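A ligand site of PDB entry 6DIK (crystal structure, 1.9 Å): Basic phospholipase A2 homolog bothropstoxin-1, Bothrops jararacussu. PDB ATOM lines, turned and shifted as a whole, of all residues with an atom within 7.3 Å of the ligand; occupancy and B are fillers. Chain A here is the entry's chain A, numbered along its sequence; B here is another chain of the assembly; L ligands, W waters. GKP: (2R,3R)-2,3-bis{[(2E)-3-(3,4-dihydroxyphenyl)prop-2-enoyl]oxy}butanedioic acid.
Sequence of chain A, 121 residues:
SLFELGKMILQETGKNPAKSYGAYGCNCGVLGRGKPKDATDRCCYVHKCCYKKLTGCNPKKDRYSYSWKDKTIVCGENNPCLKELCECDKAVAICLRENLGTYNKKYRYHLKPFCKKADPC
O of Phe 3 lies within hydrogen-bond range of O11 of the ligand, 2.9 Å away. An oxygen (O4) of the ligand lies within salt-bridge range of the side-chain amino group of Lys 7 (3.6 Å).
N of Phe 3 lies close to OG of Ser 1 (3.2 Å). O of Lys 7 sits close to OE1 of Gln 11 (3.5 Å).
Residues that only touch the ligand: Leu 2 (3.6 Å), Gly 6 (3.4 Å), Leu 10 (3.97 Å), Pro 17 (3.4 Å), Leu 111 of chain B (3.7 Å) and Pro 113 of chain B (3.4 Å). Within 4 Å of the ligand: Leu 2, Phe 3, Gly 6, Lys 7, Leu 10, Pro 17, Leu 111 of chain B and Pro 113 of chain B. The nearest printed residue that does not touch the ligand is Lys 112 of chain B (4.8 Å).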
ATOM      1  N   SER A   1     -27.711 -21.843 -28.568  1.00  0.00           N
ATOM      2  CA  SER A   1     -27.177 -21.774 -27.211  1.00  0.00           C
ATOM      3  C   SER A   1     -26.213 -20.603 -27.095  1.00  0.00           C
ATOM      4  O   SER A   1     -25.803 -20.027 -28.104  1.00  0.00           O
ATOM      5  CB  SER A   1     -26.475 -23.076 -26.821  1.00  0.00           C
ATOM      6  OG  SER A   1     -25.138 -23.092 -27.294  1.00  0.00           O
ATOM      7  N   LEU A   2     -25.839 -20.268 -25.857  1.00  0.00           N
ATOM      8  CA  LEU A   2     -24.889 -19.185 -25.646  1.00  0.00           C
ATOM      9  C   LEU A   2     -23.566 -19.428 -26.357  1.00  0.00           C
ATOM     10  O   LEU A   2     -22.863 -18.468 -26.674  1.00  0.00           O
ATOM     11  CB  LEU A   2     -24.662 -19.002 -24.139  1.00  0.00           C
ATOM     12  CG  LEU A   2     -25.957 -18.656 -23.404  1.00  0.00           C
ATOM     13  CD1 LEU A   2     -25.745 -18.584 -21.907  1.00  0.00           C
ATOM     14  CD2 LEU A   2     -26.537 -17.355 -23.926  1.00  0.00           C
ATOM     15  N   PHE A   3     -23.201 -20.691 -26.624  1.00  0.00           N
ATOM     16  CA  PHE A   3     -22.012 -20.970 -27.428  1.00  0.00           C
ATOM     17  C   PHE A   3     -22.127 -20.332 -28.810  1.00  0.00           C
ATOM     18  O   PHE A   3     -21.252 -19.574 -29.236  1.00  0.00           O
ATOM     19  CB  PHE A   3     -21.792 -22.479 -27.546  1.00  0.00           C
ATOM     20  CG  PHE A   3     -20.619 -22.854 -28.425  1.00  0.00           C
ATOM     21  CD1 PHE A   3     -19.336 -22.936 -27.889  1.00  0.00           C
ATOM     22  CD2 PHE A   3     -20.791 -23.135 -29.775  1.00  0.00           C
ATOM     23  CE1 PHE A   3     -18.261 -23.277 -28.700  1.00  0.00           C
ATOM     24  CE2 PHE A   3     -19.721 -23.471 -30.578  1.00  0.00           C
ATOM     25  CZ  PHE A   3     -18.447 -23.543 -30.042  1.00  0.00           C
ATOM     26  N   GLU A   4     -23.220 -20.636 -29.529  1.00  0.00           N
ATOM     27  CA  GLU A   4     -23.424 -20.058 -30.865  1.00  0.00           C
ATOM     28  C   GLU A   4     -23.552 -18.548 -30.804  1.00  0.00           C
ATOM     29  O   GLU A   4     -23.018 -17.836 -31.663  1.00  0.00           O
ATOM     30  CB  GLU A   4     -24.668 -20.661 -31.524  1.00  0.00           C
ATOM     31  CG  GLU A   4     -24.503 -22.098 -31.984  1.00  0.00           C
ATOM     32  CD  GLU A   4     -24.628 -23.088 -30.839  1.00  0.00           C
ATOM     33  OE1 GLU A   4     -25.259 -22.758 -29.820  1.00  0.00           O
ATOM     34  OE2 GLU A   4     -24.077 -24.200 -30.959  1.00  0.00           O
ATOM     35  N   LEU A   5     -24.281 -18.030 -29.814  1.00  0.00           N
ATOM     36  CA  LEU A   5     -24.418 -16.589 -29.667  1.00  0.00           C
ATOM     37  C   LEU A   5     -23.057 -15.923 -29.504  1.00  0.00           C
ATOM     38  O   LEU A   5     -22.761 -14.912 -30.145  1.00  0.00           O
ATOM     39  CB  LEU A   5     -25.338 -16.254 -28.491  1.00  0.00           C
ATOM     40  CG  LEU A   5     -25.403 -14.779 -28.070  1.00  0.00           C
ATOM     41  CD1 LEU A   5     -25.810 -13.931 -29.241  1.00  0.00           C
ATOM     42  CD2 LEU A   5     -26.362 -14.571 -26.893  1.00  0.00           C
ATOM     43  N   GLY A   6     -22.200 -16.491 -28.644  1.00  0.00           N
ATOM     44  CA  GLY A   6     -20.872 -15.926 -28.453  1.00  0.00           C
ATOM     45  C   GLY A   6     -20.046 -15.925 -29.721  1.00  0.00           C
ATOM     46  O   GLY A   6     -19.351 -14.954 -30.023  1.00  0.00           O
ATOM     47  N   LYS A   7     -20.104 -17.024 -30.484  1.00  0.00           N
ATOM     48  CA  LYS A   7     -19.332 -17.117 -31.715  1.00  0.00           C
ATOM     49  C   LYS A   7     -19.789 -16.085 -32.735  1.00  0.00           C
ATOM     50  O   LYS A   7     -18.964 -15.457 -33.408  1.00  0.00           O
ATOM     51  CB  LYS A   7     -19.421 -18.530 -32.297  1.00  0.00           C
ATOM     52  CG  LYS A   7     -18.473 -18.770 -33.484  1.00  0.00           C
ATOM     53  CD  LYS A   7     -18.355 -20.259 -33.812  1.00  0.00           C
ATOM     54  CE  LYS A   7     -18.760 -20.538 -35.242  1.00  0.00           C
ATOM     55  NZ  LYS A   7     -18.519 -21.960 -35.629  1.00  0.00           N
ATOM     56  N   MET A   8     -21.114 -15.881 -32.866  1.00  0.00           N
ATOM     57  CA  MET A   8     -21.622 -14.860 -33.770  1.00  0.00           C
ATOM     58  C   MET A   8     -21.120 -13.474 -33.368  1.00  0.00           C
ATOM     59  O   MET A   8     -20.706 -12.683 -34.231  1.00  0.00           O
ATOM     60  CB  MET A   8     -23.157 -14.866 -33.789  1.00  0.00           C
ATOM     61  CG  MET A   8     -23.768 -16.066 -34.471  1.00  0.00           C
ATOM     62  SD  MET A   8     -25.568 -15.878 -34.496  1.00  0.00           S
ATOM     63  CE  MET A   8     -26.043 -17.452 -35.224  1.00  0.00           C
ATOM     64  N   ILE A   9     -21.193 -13.151 -32.079  1.00  0.00           N
ATOM     65  CA  ILE A   9     -20.746 -11.840 -31.626  1.00  0.00           C
ATOM     66  C   ILE A   9     -19.272 -11.644 -31.929  1.00  0.00           C
ATOM     67  O   ILE A   9     -18.842 -10.575 -32.372  1.00  0.00           O
ATOM     68  CB  ILE A   9     -21.043 -11.667 -30.127  1.00  0.00           C
ATOM     69  CG1 ILE A   9     -22.553 -11.571 -29.878  1.00  0.00           C
ATOM     70  CG2 ILE A   9     -20.310 -10.450 -29.551  1.00  0.00           C
ATOM     71  CD1 ILE A   9     -22.935 -11.584 -28.402  1.00  0.00           C
ATOM     72  N   LEU A  10     -18.467 -12.682 -31.712  1.00  0.00           N
ATOM     73  CA  LEU A  10     -17.050 -12.589 -32.041  1.00  0.00           C
ATOM     74  C   LEU A  10     -16.850 -12.406 -33.540  1.00  0.00           C
ATOM     75  O   LEU A  10     -16.027 -11.589 -33.970  1.00  0.00           O
ATOM     76  CB  LEU A  10     -16.313 -13.831 -31.539  1.00  0.00           C
ATOM     77  CG  LEU A  10     -14.794 -13.880 -31.721  1.00  0.00           C
ATOM     78  CD1 LEU A  10     -14.113 -12.733 -30.988  1.00  0.00           C
ATOM     79  CD2 LEU A  10     -14.275 -15.214 -31.223  1.00  0.00           C
ATOM     80  N   GLN A  11     -17.605 -13.141 -34.367  1.00  0.00           N
ATOM     81  CA  GLN A  11     -17.437 -13.040 -35.812  1.00  0.00           C
ATOM     82  C   GLN A  11     -17.829 -11.660 -36.325  1.00  0.00           C
ATOM     83  O   GLN A  11     -17.179 -11.112 -37.217  1.00  0.00           O
ATOM     84  CB  GLN A  11     -18.247 -14.120 -36.517  1.00  0.00           C
ATOM     85  CG  GLN A  11     -17.666 -15.523 -36.409  1.00  0.00           C
ATOM     86  CD  GLN A  11     -18.670 -16.576 -36.837  1.00  0.00           C
ATOM     87  OE1 GLN A  11     -19.876 -16.429 -36.601  1.00  0.00           O
ATOM     88  NE2 GLN A  11     -18.187 -17.638 -37.453  1.00  0.00           N
ATOM     89  N   LYS A  15     -14.982  -8.677 -30.917  1.00  0.00           N
ATOM     90  CA  LYS A  15     -14.765  -8.447 -29.490  1.00  0.00           C
ATOM     91  C   LYS A  15     -15.006  -9.717 -28.686  1.00  0.00           C
ATOM     92  O   LYS A  15     -15.874 -10.532 -29.016  1.00  0.00           O
ATOM     93  CB  LYS A  15     -15.693  -7.350 -28.977  1.00  0.00           C
ATOM     94  CG  LYS A  15     -15.577  -6.024 -29.718  1.00  0.00           C
ATOM     95  CD  LYS A  15     -14.404  -5.201 -29.217  1.00  0.00           C
ATOM     96  CE  LYS A  15     -14.381  -3.834 -29.904  1.00  0.00           C
ATOM     97  NZ  LYS A  15     -13.222  -3.012 -29.466  1.00  0.00           N
ATOM     98  N   ASN A  16     -14.228  -9.872 -27.611  1.00  0.00           N
ATOM     99  CA  ASN A  16     -14.512 -10.899 -26.612  1.00  0.00           C
ATOM    100  C   ASN A  16     -15.932 -10.694 -26.106  1.00  0.00           C
ATOM    101  O   ASN A  16     -16.226  -9.654 -25.502  1.00  0.00           O
ATOM    102  CB  ASN A  16     -13.505 -10.808 -25.462  1.00  0.00           C
ATOM    103  CG  ASN A  16     -13.703 -11.902 -24.420  1.00  0.00           C
ATOM    104  OD1 ASN A  16     -14.778 -12.047 -23.857  1.00  0.00           O
ATOM    105  ND2 ASN A  16     -12.649 -12.668 -24.175  1.00  0.00           N
ATOM    106  N   PRO A  17     -16.842 -11.638 -26.327  1.00  0.00           N
ATOM    107  CA  PRO A  17     -18.257 -11.381 -26.005  1.00  0.00           C
ATOM    108  C   PRO A  17     -18.511 -11.179 -24.514  1.00  0.00           C
ATOM    109  O   PRO A  17     -19.310 -10.309 -24.145  1.00  0.00           O
ATOM    110  CB  PRO A  17     -18.981 -12.622 -26.530  1.00  0.00           C
ATOM    111  CG  PRO A  17     -18.023 -13.259 -27.493  1.00  0.00           C
ATOM    112  CD  PRO A  17     -16.653 -12.948 -26.987  1.00  0.00           C
ATOM    113  N   ALA A  18     -17.855 -11.948 -23.652  1.00  0.00           N
ATOM    114  CA  ALA A  18     -18.098 -11.783 -22.225  1.00  0.00           C
ATOM    115  C   ALA A  18     -17.566 -10.444 -21.729  1.00  0.00           C
ATOM    116  O   ALA A  18     -18.207  -9.772 -20.923  1.00  0.00           O
ATOM    117  CB  ALA A  18     -17.481 -12.938 -21.433  1.00  0.00           C
ATOM    118  N   TYR A  66     -25.002 -23.011 -37.974  1.00  0.00           N
ATOM    119  CA  TYR A  66     -25.058 -21.900 -38.916  1.00  0.00           C
ATOM    120  C   TYR A  66     -23.726 -21.835 -39.667  1.00  0.00           C
ATOM    121  O   TYR A  66     -22.745 -22.480 -39.293  1.00  0.00           O
ATOM    122  CB  TYR A  66     -25.381 -20.571 -38.223  1.00  0.00           C
ATOM    123  CG  TYR A  66     -24.242 -19.957 -37.442  1.00  0.00           C
ATOM    124  CD1 TYR A  66     -24.032 -20.297 -36.112  1.00  0.00           C
ATOM    125  CD2 TYR A  66     -23.379 -19.032 -38.023  1.00  0.00           C
ATOM    126  CE1 TYR A  66     -23.001 -19.734 -35.384  1.00  0.00           C
ATOM    127  CE2 TYR A  66     -22.343 -18.473 -37.302  1.00  0.00           C
ATOM    128  CZ  TYR A  66     -22.153 -18.824 -35.975  1.00  0.00           C
ATOM    129  OH  TYR A  66     -21.141 -18.271 -35.250  1.00  0.00           O
ATOM    130  N   TYR B 109     -12.966 -13.665 -18.607  1.00  0.00           N
ATOM    131  CA  TYR B 109     -13.395 -13.658 -20.000  1.00  0.00           C
ATOM    132  C   TYR B 109     -12.745 -14.774 -20.808  1.00  0.00           C
ATOM    133  O   TYR B 109     -12.491 -14.640 -21.996  1.00  0.00           O
ATOM    134  CB  TYR B 109     -13.136 -12.295 -20.671  1.00  0.00           C
ATOM    135  CG  TYR B 109     -13.382 -11.145 -19.725  1.00  0.00           C
ATOM    136  CD1 TYR B 109     -14.644 -10.925 -19.192  1.00  0.00           C
ATOM    137  CD2 TYR B 109     -12.340 -10.310 -19.335  1.00  0.00           C
ATOM    138  CE1 TYR B 109     -14.871  -9.886 -18.304  1.00  0.00           C
ATOM    139  CE2 TYR B 109     -12.562  -9.276 -18.454  1.00  0.00           C
ATOM    140  CZ  TYR B 109     -13.828  -9.059 -17.950  1.00  0.00           C
ATOM    141  OH  TYR B 109     -14.063  -8.028 -17.074  1.00  0.00           O
ATOM    142  N   HIS B 110     -12.470 -15.895 -20.141  1.00  0.00           N
ATOM    143  CA  HIS B 110     -11.943 -17.062 -20.819  1.00  0.00           C
ATOM    144  C   HIS B 110     -12.957 -17.605 -21.824  1.00  0.00           C
ATOM    145  O   HIS B 110     -14.149 -17.712 -21.520  1.00  0.00           O
ATOM    146  CB  HIS B 110     -11.578 -18.134 -19.796  1.00  0.00           C
ATOM    147  CG  HIS B 110     -10.804 -19.281 -20.362  1.00  0.00           C
ATOM    148  ND1 HIS B 110      -9.425 -19.296 -20.390  1.00  0.00           N
ATOM    149  CD2 HIS B 110     -11.206 -20.439 -20.926  1.00  0.00           C
ATOM    150  CE1 HIS B 110      -9.011 -20.419 -20.947  1.00  0.00           C
ATOM    151  NE2 HIS B 110     -10.073 -21.131 -21.287  1.00  0.00           N
ATOM    152  N   LEU B 111     -12.487 -17.950 -23.019  1.00  0.00           N
ATOM    153  CA  LEU B 111     -13.350 -18.373 -24.106  1.00  0.00           C
ATOM    154  C   LEU B 111     -13.632 -19.871 -24.045  1.00  0.00           C
ATOM    155  O   LEU B 111     -12.746 -20.678 -23.743  1.00  0.00           O
ATOM    156  CB  LEU B 111     -12.727 -18.020 -25.459  1.00  0.00           C
ATOM    157  CG  LEU B 111     -12.610 -16.543 -25.803  1.00  0.00           C
ATOM    158  CD1 LEU B 111     -12.012 -16.351 -27.189  1.00  0.00           C
ATOM    159  CD2 LEU B 111     -13.969 -15.868 -25.709  1.00  0.00           C
ATOM    160  N   LYS B 112     -14.857 -20.247 -24.380  1.00  0.00           N
ATOM    161  CA  LYS B 112     -15.289 -21.644 -24.341  1.00  0.00           C
ATOM    162  C   LYS B 112     -14.490 -22.621 -25.217  1.00  0.00           C
ATOM    163  O   LYS B 112     -14.150 -23.696 -24.764  1.00  0.00           O
ATOM    164  CB  LYS B 112     -16.768 -21.764 -24.667  1.00  0.00           C
ATOM    165  CG  LYS B 112     -17.568 -22.529 -23.635  1.00  0.00           C
ATOM    166  N   PRO B 113     -14.234 -22.259 -26.474  1.00  0.00           N
ATOM    167  CA  PRO B 113     -13.473 -23.208 -27.311  1.00  0.00           C
ATOM    168  C   PRO B 113     -12.122 -23.598 -26.731  1.00  0.00           C
ATOM    169  O   PRO B 113     -11.529 -24.586 -27.175  1.00  0.00           O
ATOM    170  CB  PRO B 113     -13.312 -22.469 -28.649  1.00  0.00           C
ATOM    171  CG  PRO B 113     -13.623 -21.043 -28.346  1.00  0.00           C
ATOM    172  CD  PRO B 113     -14.648 -21.081 -27.261  1.00  0.00           C
ATOM    173  N   PHE B 114     -11.613 -22.853 -25.740  1.00  0.00           N
ATOM    174  CA  PHE B 114     -10.354 -23.160 -25.096  1.00  0.00           C
ATOM    175  C   PHE B 114     -10.537 -23.912 -23.776  1.00  0.00           C
ATOM    176  O   PHE B 114      -9.663 -23.871 -22.910  1.00  0.00           O
ATOM    177  CB  PHE B 114      -9.546 -21.873 -24.895  1.00  0.00           C
ATOM    178  CG  PHE B 114      -9.267 -21.145 -26.185  1.00  0.00           C
ATOM    179  CD1 PHE B 114      -8.978 -21.851 -27.346  1.00  0.00           C
ATOM    180  CD2 PHE B 114      -9.297 -19.760 -26.235  1.00  0.00           C
ATOM    181  CE1 PHE B 114      -8.726 -21.190 -28.547  1.00  0.00           C
ATOM    182  CE2 PHE B 114      -9.042 -19.087 -27.431  1.00  0.00           C
ATOM    183  CZ  PHE B 114      -8.753 -19.804 -28.583  1.00  0.00           C
HETATM  184  C1  GKP L   1     -15.936 -18.646 -29.578  1.00  0.00           C
HETATM  185  C10 GKP L   1     -14.093 -23.413 -33.663  1.00  0.00           C
HETATM  186  C11 GKP L   1     -14.567 -23.138 -35.071  1.00  0.00           C
HETATM  187  C12 GKP L   1     -12.667 -23.937 -33.664  1.00  0.00           C
HETATM  188  C13 GKP L   1     -10.549 -23.422 -34.617  1.00  0.00           C
HETATM  189  C14 GKP L   1      -9.485 -22.470 -34.993  1.00  0.00           C
HETATM  190  C15 GKP L   1      -8.243 -22.909 -35.175  1.00  0.00           C
HETATM  191  C16 GKP L   1      -7.164 -21.952 -35.531  1.00  0.00           C
HETATM  192  C17 GKP L   1      -5.929 -22.434 -35.945  1.00  0.00           C
HETATM  193  C18 GKP L   1      -4.914 -21.550 -36.272  1.00  0.00           C
HETATM  194  C19 GKP L   1      -5.173 -20.093 -36.180  1.00  0.00           C
HETATM  195  C2  GKP L   1     -16.093 -17.618 -28.642  1.00  0.00           C
HETATM  196  C20 GKP L   1      -6.419 -19.656 -35.768  1.00  0.00           C
HETATM  197  C21 GKP L   1      -7.404 -20.580 -35.435  1.00  0.00           C
HETATM  198  C22 GKP L   1     -12.289 -24.246 -32.246  1.00  0.00           C
HETATM  199  C3  GKP L   1     -17.225 -17.593 -27.840  1.00  0.00           C
HETATM  200  C4  GKP L   1     -18.241 -18.660 -27.993  1.00  0.00           C
HETATM  201  C5  GKP L   1     -18.045 -19.655 -28.930  1.00  0.00           C
HETATM  202  C6  GKP L   1     -16.895 -19.640 -29.723  1.00  0.00           C
HETATM  203  C7  GKP L   1     -16.711 -20.729 -30.709  1.00  0.00           C
HETATM  204  C8  GKP L   1     -15.598 -20.814 -31.424  1.00  0.00           C
HETATM  205  C9  GKP L   1     -15.443 -21.915 -32.390  1.00  0.00           C
HETATM  206  O1  GKP L   1     -16.392 -22.574 -32.771  1.00  0.00           O
HETATM  207  O10 GKP L   1     -12.494 -25.462 -31.745  1.00  0.00           O
HETATM  208  O11 GKP L   1     -19.350 -18.660 -27.214  1.00  0.00           O
HETATM  209  O12 GKP L   1     -17.406 -16.601 -26.919  1.00  0.00           O
HETATM  210  O2  GKP L   1     -14.118 -22.215 -32.910  1.00  0.00           O
HETATM  211  O3  GKP L   1     -14.139 -22.191 -35.712  1.00  0.00           O
HETATM  212  O4  GKP L   1     -15.465 -23.935 -35.636  1.00  0.00           O
HETATM  213  O5  GKP L   1     -11.811 -22.913 -34.130  1.00  0.00           O
HETATM  214  O6  GKP L   1     -10.376 -24.626 -34.710  1.00  0.00           O
HETATM  215  O7  GKP L   1      -4.192 -19.205 -36.503  1.00  0.00           O
HETATM  216  O8  GKP L   1      -3.707 -22.020 -36.683  1.00  0.00           O
HETATM  217  O9  GKP L   1     -11.799 -23.382 -31.542  1.00  0.00           O
HETATM  218  O   HOH W   1      -3.191 -24.331 -35.496  1.00  0.00           O
HETATM  219  O   HOH W   2     -19.784 -16.992 -25.185  1.00  0.00           O
